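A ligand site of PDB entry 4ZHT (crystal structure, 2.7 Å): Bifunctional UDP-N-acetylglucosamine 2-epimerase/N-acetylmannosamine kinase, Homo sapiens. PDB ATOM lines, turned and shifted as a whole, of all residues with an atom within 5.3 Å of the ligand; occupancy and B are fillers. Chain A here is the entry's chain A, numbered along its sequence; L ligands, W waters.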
ATOM      1  N   ASN A  18      11.206   2.987  -0.920  1.00  0.00           N
ATOM      2  CA  ASN A  18      12.316   2.063  -1.051  1.00  0.00           C
ATOM      3  C   ASN A  18      13.449   2.801  -1.725  1.00  0.00           C
ATOM      4  O   ASN A  18      13.200   3.733  -2.503  1.00  0.00           O
ATOM      5  CB  ASN A  18      11.875   0.845  -1.893  1.00  0.00           C
ATOM      6  CG  ASN A  18      12.923  -0.278  -1.953  1.00  0.00           C
ATOM      7  OD1 ASN A  18      13.932  -0.165  -2.670  1.00  0.00           O
ATOM      8  ND2 ASN A  18      12.698  -1.346  -1.195  1.00  0.00           N
ATOM      9  N   ARG A  19      14.686   2.412  -1.423  1.00  0.00           N
ATOM     10  CA  ARG A  19      15.847   2.968  -2.093  1.00  0.00           C
ATOM     11  C   ARG A  19      15.712   2.898  -3.622  1.00  0.00           C
ATOM     12  O   ARG A  19      16.361   3.670  -4.366  1.00  0.00           O
ATOM     13  CB  ARG A  19      17.101   2.219  -1.701  1.00  0.00           C
ATOM     14  CG  ARG A  19      17.350   1.052  -2.653  1.00  0.00           C
ATOM     15  CD  ARG A  19      18.622   0.326  -2.411  1.00  0.00           C
ATOM     16  NE  ARG A  19      18.566  -0.984  -3.026  1.00  0.00           N
ATOM     17  CZ  ARG A  19      19.249  -2.032  -2.603  1.00  0.00           C
ATOM     18  NH1 ARG A  19      20.090  -1.923  -1.581  1.00  0.00           N
ATOM     19  NH2 ARG A  19      19.104  -3.193  -3.206  1.00  0.00           N
ATOM     20  N   ALA A  20      14.938   1.920  -4.110  1.00  0.00           N
ATOM     21  CA  ALA A  20      14.776   1.700  -5.552  1.00  0.00           C
ATOM     22  C   ALA A  20      14.050   2.837  -6.229  1.00  0.00           C
ATOM     23  O   ALA A  20      14.263   3.059  -7.407  1.00  0.00           O
ATOM     24  CB  ALA A  20      14.061   0.387  -5.829  1.00  0.00           C
ATOM     25  N   SER A  23      16.517   6.586  -5.421  1.00  0.00           N
ATOM     26  CA  SER A  23      17.626   6.931  -6.317  1.00  0.00           C
ATOM     27  C   SER A  23      17.172   7.794  -7.510  1.00  0.00           C
ATOM     28  O   SER A  23      17.954   8.579  -8.041  1.00  0.00           O
ATOM     29  CB  SER A  23      18.382   5.697  -6.801  1.00  0.00           C
ATOM     30  OG  SER A  23      17.614   4.928  -7.717  1.00  0.00           O
ATOM     31  N   LYS A  24      15.915   7.646  -7.910  1.00  0.00           N
ATOM     32  CA  LYS A  24      15.378   8.331  -9.066  1.00  0.00           C
ATOM     33  C   LYS A  24      14.443   9.440  -8.688  1.00  0.00           C
ATOM     34  O   LYS A  24      14.123  10.267  -9.529  1.00  0.00           O
ATOM     35  CB  LYS A  24      14.676   7.324  -9.977  1.00  0.00           C
ATOM     36  CG  LYS A  24      15.639   6.331 -10.608  1.00  0.00           C
ATOM     37  CD  LYS A  24      14.933   5.083 -11.099  1.00  0.00           C
ATOM     38  CE  LYS A  24      15.850   4.039 -11.705  1.00  0.00           C
ATOM     39  NZ  LYS A  24      16.911   3.576 -10.779  1.00  0.00           N
ATOM     40  N   ASP A 112       7.406   0.558 -10.522  1.00  0.00           N
ATOM     41  CA  ASP A 112       6.643  -0.663 -10.796  1.00  0.00           C
ATOM     42  C   ASP A 112       6.392  -1.580  -9.601  1.00  0.00           C
ATOM     43  O   ASP A 112       5.905  -2.671  -9.743  1.00  0.00           O
ATOM     44  CB  ASP A 112       7.390  -1.445 -11.914  1.00  0.00           C
ATOM     45  CG  ASP A 112       8.865  -1.809 -11.559  1.00  0.00           C
ATOM     46  OD1 ASP A 112       9.287  -1.673 -10.393  1.00  0.00           O
ATOM     47  OD2 ASP A 112       9.630  -2.251 -12.442  1.00  0.00           O
ATOM     48  N   ARG A 113       6.722  -1.123  -8.415  1.00  0.00           N
ATOM     49  CA  ARG A 113       6.564  -1.925  -7.213  1.00  0.00           C
ATOM     50  C   ARG A 113       5.151  -1.815  -6.607  1.00  0.00           C
ATOM     51  O   ARG A 113       4.438  -0.833  -6.826  1.00  0.00           O
ATOM     52  CB  ARG A 113       7.607  -1.525  -6.198  1.00  0.00           C
ATOM     53  CG  ARG A 113       8.975  -2.018  -6.599  1.00  0.00           C
ATOM     54  CD  ARG A 113      10.079  -1.451  -5.744  1.00  0.00           C
ATOM     55  NE  ARG A 113      11.321  -2.081  -6.133  1.00  0.00           N
ATOM     56  CZ  ARG A 113      12.059  -2.899  -5.382  1.00  0.00           C
ATOM     57  NH1 ARG A 113      11.744  -3.191  -4.116  1.00  0.00           N
ATOM     58  NH2 ARG A 113      13.182  -3.426  -5.918  1.00  0.00           N
ATOM     59  N   LEU A 218      23.989  -8.590  -7.185  1.00  0.00           N
ATOM     60  CA  LEU A 218      22.700  -8.099  -6.732  1.00  0.00           C
ATOM     61  C   LEU A 218      21.616  -8.848  -7.474  1.00  0.00           C
ATOM     62  O   LEU A 218      21.348  -8.599  -8.665  1.00  0.00           O
ATOM     63  CB  LEU A 218      22.629  -6.598  -6.984  1.00  0.00           C
ATOM     64  CG  LEU A 218      21.379  -5.768  -6.715  1.00  0.00           C
ATOM     65  CD1 LEU A 218      20.893  -5.901  -5.277  1.00  0.00           C
ATOM     66  CD2 LEU A 218      21.690  -4.315  -7.015  1.00  0.00           C
ATOM     67  N   HIS A 220      17.592 -10.484  -7.154  1.00  0.00           N
ATOM     68  CA  HIS A 220      16.323 -10.410  -6.505  1.00  0.00           C
ATOM     69  C   HIS A 220      15.484 -11.606  -6.843  1.00  0.00           C
ATOM     70  O   HIS A 220      15.559 -12.114  -7.940  1.00  0.00           O
ATOM     71  CB  HIS A 220      15.559  -9.178  -6.970  1.00  0.00           C
ATOM     72  CG  HIS A 220      16.307  -7.908  -6.786  1.00  0.00           C
ATOM     73  ND1 HIS A 220      16.916  -7.585  -5.594  1.00  0.00           N
ATOM     74  CD2 HIS A 220      16.571  -6.887  -7.633  1.00  0.00           C
ATOM     75  CE1 HIS A 220      17.533  -6.426  -5.706  1.00  0.00           C
ATOM     76  NE2 HIS A 220      17.324  -5.980  -6.937  1.00  0.00           N
ATOM     77  N   LEU A 250      24.858  -7.761  -2.290  1.00  0.00           N
ATOM     78  CA  LEU A 250      23.751  -6.993  -1.751  1.00  0.00           C
ATOM     79  C   LEU A 250      22.617  -7.960  -1.411  1.00  0.00           C
ATOM     80  O   LEU A 250      22.287  -8.795  -2.200  1.00  0.00           O
ATOM     81  CB  LEU A 250      23.227  -5.996  -2.776  1.00  0.00           C
ATOM     82  CG  LEU A 250      23.896  -4.656  -2.952  1.00  0.00           C
ATOM     83  CD1 LEU A 250      23.615  -3.786  -1.749  1.00  0.00           C
ATOM     84  CD2 LEU A 250      25.392  -4.784  -3.211  1.00  0.00           C
ATOM     85  N   ASN A 253      16.141  -7.350  -2.483  1.00  0.00           N
ATOM     86  CA  ASN A 253      15.300  -6.183  -2.342  1.00  0.00           C
ATOM     87  C   ASN A 253      13.990  -6.308  -3.142  1.00  0.00           C
ATOM     88  O   ASN A 253      13.511  -5.316  -3.715  1.00  0.00           O
ATOM     89  CB  ASN A 253      16.049  -4.953  -2.819  1.00  0.00           C
ATOM     90  CG  ASN A 253      15.337  -3.676  -2.473  1.00  0.00           C
ATOM     91  OD1 ASN A 253      14.758  -3.559  -1.404  1.00  0.00           O
ATOM     92  ND2 ASN A 253      15.418  -2.689  -3.366  1.00  0.00           N
ATOM     93  N   ILE A 254      13.474  -7.532  -3.244  1.00  0.00           N
ATOM     94  CA  ILE A 254      12.060  -7.757  -3.505  1.00  0.00           C
ATOM     95  C   ILE A 254      11.616  -8.561  -2.315  1.00  0.00           C
ATOM     96  O   ILE A 254      12.253  -9.542  -1.954  1.00  0.00           O
ATOM     97  CB  ILE A 254      11.800  -8.559  -4.800  1.00  0.00           C
ATOM     98  CG1 ILE A 254      12.243  -7.770  -6.045  1.00  0.00           C
ATOM     99  CG2 ILE A 254      10.338  -8.954  -4.927  1.00  0.00           C
ATOM    100  CD1 ILE A 254      11.388  -6.552  -6.377  1.00  0.00           C
ATOM    101  N   LYS A 280      23.342  -4.512   3.061  1.00  0.00           N
ATOM    102  CA  LYS A 280      21.944  -4.224   2.751  1.00  0.00           C
ATOM    103  C   LYS A 280      21.861  -3.072   1.773  1.00  0.00           C
ATOM    104  O   LYS A 280      21.199  -3.172   0.764  1.00  0.00           O
ATOM    105  CB  LYS A 280      21.158  -3.862   4.012  1.00  0.00           C
ATOM    106  CG  LYS A 280      21.094  -4.985   5.013  1.00  0.00           C
ATOM    107  CD  LYS A 280      20.513  -4.557   6.352  1.00  0.00           C
ATOM    108  CE  LYS A 280      20.255  -5.768   7.238  1.00  0.00           C
ATOM    109  NZ  LYS A 280      19.908  -5.378   8.632  1.00  0.00           N
ATOM    110  N   HIS A 281      22.538  -1.984   2.080  1.00  0.00           N
ATOM    111  CA  HIS A 281      22.473  -0.809   1.222  1.00  0.00           C
ATOM    112  C   HIS A 281      23.751  -0.016   1.262  1.00  0.00           C
ATOM    113  O   HIS A 281      24.251   0.319   2.329  1.00  0.00           O
ATOM    114  CB  HIS A 281      21.305   0.078   1.654  1.00  0.00           C
ATOM    115  CG  HIS A 281      21.183   1.331   0.852  1.00  0.00           C
ATOM    116  ND1 HIS A 281      20.808   1.325  -0.478  1.00  0.00           N
ATOM    117  CD2 HIS A 281      21.381   2.624   1.169  1.00  0.00           C
ATOM    118  CE1 HIS A 281      20.764   2.573  -0.936  1.00  0.00           C
ATOM    119  NE2 HIS A 281      21.108   3.380   0.053  1.00  0.00           N
ATOM    120  N   VAL A 282      24.244   0.309   0.073  1.00  0.00           N
ATOM    121  CA  VAL A 282      25.349   1.250  -0.145  1.00  0.00           C
ATOM    122  C   VAL A 282      24.743   2.562  -0.591  1.00  0.00           C
ATOM    123  O   VAL A 282      23.997   2.598  -1.585  1.00  0.00           O
ATOM    124  CB  VAL A 282      26.290   0.766  -1.295  1.00  0.00           C
ATOM    125  CG1 VAL A 282      27.456   1.720  -1.460  1.00  0.00           C
ATOM    126  CG2 VAL A 282      26.798  -0.632  -1.005  1.00  0.00           C
ATOM    127  N   PRO A 283      25.102   3.658   0.081  1.00  0.00           N
ATOM    128  CA  PRO A 283      24.619   4.969  -0.370  1.00  0.00           C
ATOM    129  C   PRO A 283      24.841   5.226  -1.873  1.00  0.00           C
ATOM    130  O   PRO A 283      25.932   4.977  -2.399  1.00  0.00           O
ATOM    131  CB  PRO A 283      25.409   5.969   0.508  1.00  0.00           C
ATOM    132  CG  PRO A 283      25.933   5.192   1.664  1.00  0.00           C
ATOM    133  CD  PRO A 283      25.874   3.722   1.329  1.00  0.00           C
ATOM    134  N   PHE A 284      23.793   5.728  -2.525  1.00  0.00           N
ATOM    135  CA  PHE A 284      23.716   5.819  -3.967  1.00  0.00           C
ATOM    136  C   PHE A 284      24.971   6.424  -4.614  1.00  0.00           C
ATOM    137  O   PHE A 284      25.505   5.859  -5.551  1.00  0.00           O
ATOM    138  CB  PHE A 284      22.459   6.573  -4.395  1.00  0.00           C
ATOM    139  CG  PHE A 284      22.258   6.651  -5.889  1.00  0.00           C
ATOM    140  CD1 PHE A 284      22.252   5.504  -6.669  1.00  0.00           C
ATOM    141  CD2 PHE A 284      22.039   7.888  -6.525  1.00  0.00           C
ATOM    142  CE1 PHE A 284      22.071   5.573  -8.051  1.00  0.00           C
ATOM    143  CE2 PHE A 284      21.838   7.952  -7.895  1.00  0.00           C
ATOM    144  CZ  PHE A 284      21.851   6.807  -8.665  1.00  0.00           C
ATOM    145  N   PHE A 287      27.620   3.978  -4.302  1.00  0.00           N
ATOM    146  CA  PHE A 287      27.291   2.821  -5.101  1.00  0.00           C
ATOM    147  C   PHE A 287      27.634   3.031  -6.572  1.00  0.00           C
ATOM    148  O   PHE A 287      28.052   2.083  -7.261  1.00  0.00           O
ATOM    149  CB  PHE A 287      25.811   2.483  -4.925  1.00  0.00           C
ATOM    150  CG  PHE A 287      25.415   1.169  -5.545  1.00  0.00           C
ATOM    151  CD1 PHE A 287      25.907  -0.025  -5.019  1.00  0.00           C
ATOM    152  CD2 PHE A 287      24.574   1.124  -6.651  1.00  0.00           C
ATOM    153  CE1 PHE A 287      25.543  -1.250  -5.584  1.00  0.00           C
ATOM    154  CE2 PHE A 287      24.212  -0.082  -7.204  1.00  0.00           C
ATOM    155  CZ  PHE A 287      24.691  -1.272  -6.673  1.00  0.00           C
ATOM    156  N   ASN A 300      20.219  -9.550 -11.365  1.00  0.00           N
ATOM    157  CA  ASN A 300      19.095  -9.088 -12.177  1.00  0.00           C
ATOM    158  C   ASN A 300      18.563  -7.697 -11.803  1.00  0.00           C
ATOM    159  O   ASN A 300      17.389  -7.406 -12.009  1.00  0.00           O
ATOM    160  CB  ASN A 300      17.984 -10.126 -12.114  1.00  0.00           C
ATOM    161  CG  ASN A 300      17.436 -10.326 -10.726  1.00  0.00           C
ATOM    162  OD1 ASN A 300      17.742  -9.570  -9.821  1.00  0.00           O
ATOM    163  ND2 ASN A 300      16.641 -11.332 -10.547  1.00  0.00           N
ATOM    164  N   SER A 301      19.438  -6.859 -11.253  1.00  0.00           N
ATOM    165  CA  SER A 301      19.079  -5.503 -10.934  1.00  0.00           C
ATOM    166  C   SER A 301      18.714  -4.750 -12.198  1.00  0.00           C
ATOM    167  O   SER A 301      19.224  -5.031 -13.291  1.00  0.00           O
ATOM    168  CB  SER A 301      20.255  -4.815 -10.230  1.00  0.00           C
ATOM    169  OG  SER A 301      19.864  -3.572  -9.672  1.00  0.00           O
ATOM    170  N   SER A 302      17.871  -3.744 -12.047  1.00  0.00           N
ATOM    171  CA  SER A 302      17.630  -2.779 -13.127  1.00  0.00           C
ATOM    172  C   SER A 302      18.878  -1.916 -13.401  1.00  0.00           C
ATOM    173  O   SER A 302      19.025  -1.391 -14.488  1.00  0.00           O
ATOM    174  CB  SER A 302      16.465  -1.860 -12.786  1.00  0.00           C
ATOM    175  OG  SER A 302      16.853  -0.892 -11.842  1.00  0.00           O
ATOM    176  N   CYS A 303      19.713  -1.721 -12.366  1.00  0.00           N
ATOM    177  CA  CYS A 303      20.956  -1.001 -12.498  1.00  0.00           C
ATOM    178  C   CYS A 303      21.821  -1.627 -13.576  1.00  0.00           C
ATOM    179  O   CYS A 303      22.414  -0.931 -14.411  1.00  0.00           O
ATOM    180  CB  CYS A 303      21.693  -0.979 -11.152  1.00  0.00           C
ATOM    181  SG  CYS A 303      23.330  -0.223 -11.264  1.00  0.00           S
ATOM    182  N   GLU A 307      21.612   1.416 -15.852  1.00  0.00           N
ATOM    183  CA  GLU A 307      22.499   2.445 -15.332  1.00  0.00           C
ATOM    184  C   GLU A 307      23.959   2.216 -15.715  1.00  0.00           C
ATOM    185  O   GLU A 307      24.547   3.068 -16.395  1.00  0.00           O
ATOM    186  CB  GLU A 307      22.333   2.562 -13.814  1.00  0.00           C
ATOM    187  CG  GLU A 307      20.952   3.059 -13.409  1.00  0.00           C
ATOM    188  CD  GLU A 307      20.727   3.068 -11.892  1.00  0.00           C
ATOM    189  OE1 GLU A 307      21.726   3.085 -11.121  1.00  0.00           O
ATOM    190  OE2 GLU A 307      19.538   3.046 -11.488  1.00  0.00           O
ATOM    191  N   ARG A 321      13.868 -11.923 -15.040  1.00  0.00           N
ATOM    192  CA  ARG A 321      13.705 -10.524 -14.690  1.00  0.00           C
ATOM    193  C   ARG A 321      14.642  -9.711 -15.572  1.00  0.00           C
ATOM    194  O   ARG A 321      15.862 -10.006 -15.656  1.00  0.00           O
ATOM    195  CB  ARG A 321      14.047 -10.308 -13.223  1.00  0.00           C
ATOM    196  CG  ARG A 321      13.661  -8.933 -12.705  1.00  0.00           C
ATOM    197  CD  ARG A 321      14.105  -8.774 -11.249  1.00  0.00           C
ATOM    198  NE  ARG A 321      13.411  -7.667 -10.600  1.00  0.00           N
ATOM    199  CZ  ARG A 321      13.915  -6.463 -10.288  1.00  0.00           C
ATOM    200  NH1 ARG A 321      15.170  -6.117 -10.557  1.00  0.00           N
ATOM    201  NH2 ARG A 321      13.145  -5.581  -9.675  1.00  0.00           N
ATOM    202  N   GLN A 322      14.073  -8.690 -16.205  1.00  0.00           N
ATOM    203  CA  GLN A 322      14.710  -7.809 -17.199  1.00  0.00           C
ATOM    204  C   GLN A 322      14.648  -8.292 -18.628  1.00  0.00           C
ATOM    205  O   GLN A 322      15.214  -7.646 -19.497  1.00  0.00           O
ATOM    206  CB  GLN A 322      16.162  -7.415 -16.852  1.00  0.00           C
ATOM    207  CG  GLN A 322      16.413  -6.925 -15.428  1.00  0.00           C
ATOM    208  CD  GLN A 322      15.530  -5.764 -15.015  1.00  0.00           C
ATOM    209  OE1 GLN A 322      14.898  -5.114 -15.846  1.00  0.00           O
ATOM    210  NE2 GLN A 322      15.506  -5.480 -13.717  1.00  0.00           N
HETATM  211  N1  LIG L   1      21.217   0.896  -5.352  1.00  0.00           N
HETATM  212  C1  LIG L   1      21.767   1.733  -4.339  1.00  0.00           C
HETATM  213  N2  LIG L   1      22.528   1.203  -3.382  1.00  0.00           N
HETATM  214  C2  LIG L   1      22.749  -0.125  -3.335  1.00  0.00           C
HETATM  215  C3  LIG L   1      22.218  -0.964  -4.294  1.00  0.00           C
HETATM  216  C4  LIG L   1      21.424  -0.418  -5.291  1.00  0.00           C
HETATM  217  O1  LIG L   1      21.555   2.966  -4.341  1.00  0.00           O
HETATM  218  O2  LIG L   1      23.453  -0.627  -2.432  1.00  0.00           O
HETATM  219  C5  LIG L   1      20.360   1.460  -6.395  1.00  0.00           C
HETATM  220  C6  LIG L   1      20.555   1.070  -7.867  1.00  0.00           C
HETATM  221  O3  LIG L   1      21.624   1.727  -8.557  1.00  0.00           O
HETATM  222  C7  LIG L   1      19.187   1.440  -8.415  1.00  0.00           C
HETATM  223  C8  LIG L   1      18.235   1.187  -7.242  1.00  0.00           C
HETATM  224  O4  LIG L   1      19.069   0.964  -6.111  1.00  0.00           O
HETATM  225  O5  LIG L   1      19.153   2.834  -8.776  1.00  0.00           O
HETATM  226  C9  LIG L   1      17.347  -0.037  -7.378  1.00  0.00           C
HETATM  227  O6  LIG L   1      18.114  -1.238  -7.364  1.00  0.00           O
HETATM  228  P1  LIG L   1      17.482  -2.615  -6.816  1.00  0.00           P
HETATM  229  O7  LIG L   1      18.288  -3.727  -7.407  1.00  0.00           O
HETATM  230  O8  LIG L   1      17.421  -2.588  -5.317  1.00  0.00           O
HETATM  231  O9  LIG L   1      15.986  -2.519  -7.366  1.00  0.00           O
HETATM  232  P2  LIG L   1      15.510  -2.701  -8.894  1.00  0.00           P
HETATM  233  O10 LIG L   1      16.396  -3.840  -9.318  1.00  0.00           O
HETATM  234  O11 LIG L   1      15.708  -1.392  -9.614  1.00  0.00           O
HETATM  235  O12 LIG L   1      14.016  -2.960  -8.810  1.00  0.00           O
HETATM  236  O   HOH W   1      14.035   0.848 -10.008  1.00  0.00           O
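N of Asn 253 lies within hydrogen-bond range of ND1 of His 220, at 3.2 Å.
The side-chain amide oxygen (OD1) of Asn 300 lies within hydrogen-bond range of the backbone NH (N) of His 220, 2.8 Å away.
The side-chain carboxylate of Glu 307 is in salt-bridge range of the side-chain amino group of Lys 24 (2.8 Å).
OG of Ser 301 sits close to N of Cys 303.
NH1 of Arg 113 sits at hydrogen-bond distance from O of Asn 253 (2.8 Å).
The side-chain amide nitrogen of Asn 253 lies within hydrogen-bond range of the side-chain amide oxygen of Asn 18 (3.0 Å).
The guanidinium group of Arg 321 lies within hydrogen-bond range of the backbone carbonyl oxygen of Asn 300, at 2.9 Å.
The side-chain amide nitrogen of Gln 322 sits close to the guanidinium group of Arg 321 (3.2 Å).
Merely in contact with the ligand: Ala 20 (3.6 Å), Leu 218 (3.5 Å), Leu 250 (3.2 Å), Phe 284 (3.5 Å) and Phe 287 (3.4 Å).
Hydrophobic or aromatic side chains within 4 Å of the ligand: Ala 20, Leu 218, His 220, Leu 250, His 281, Val 282, Phe 284 and Phe 287.
18 residues have an atom within 4 Å of the ligand: Arg 19, Ala 20, Ser 23, Lys 24, Arg 113, Leu 218, His 220, Leu 250, Asn 253, His 281, Val 282, Phe 284, Phe 287, Ser 301, Ser 302, Cys 303, Glu 307 and Arg 321.
NE2 of His 220 sits at hydrogen-bond distance from O7 of the ligand.
N of Ser 302 sits at hydrogen-bond distance from O10 of the ligand (3.1 Å).
OG of Ser 302 sits at hydrogen-bond distance from O11 of the ligand.
N of Val 282 sits at hydrogen-bond distance from O2 of the ligand (2.8 Å).
A nitrogen (N2) of the ligand lies within hydrogen-bond range of the backbone carbonyl oxygen (O) of Val 282, 2.7 Å away.
OE2 of Glu 307 lies within hydrogen-bond range of O5 of the ligand.
OG of Ser 301 is in hydrogen-bond range of O7 of the ligand (2.8 Å).
The guanidinium group (NH2) of Arg 19 is in salt-bridge range of an oxygen (O8) of the ligand (2.8 Å).
The side-chain amide nitrogen of Asn 253 lies within hydrogen-bond range of an oxygen (O8) of the ligand.
OG of Ser 23 lies within hydrogen-bond range of O5 of the ligand.
The guanidinium group (NH1) of Arg 321 is in salt-bridge range of an oxygen (O10) of the ligand, 2.9 Å away.
NH2 of Arg 113 lies within salt-bridge range of O12 of the ligand, 3.0 Å away.
O5 of the ligand lies within hydrogen-bond range of NZ of Lys 24, at 3.1 Å.
A ring nitrogen (ND1) of His 281 sits close to a nitrogen (N2) of the ligand (3.4 Å).
The side-chain sulfur (SG) of Cys 303 sits at hydrogen-bond distance from an oxygen (O3) of the ligand, 3.7 Å away.
Water W1 bridges O11 of the ligand and O of Ala 20.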
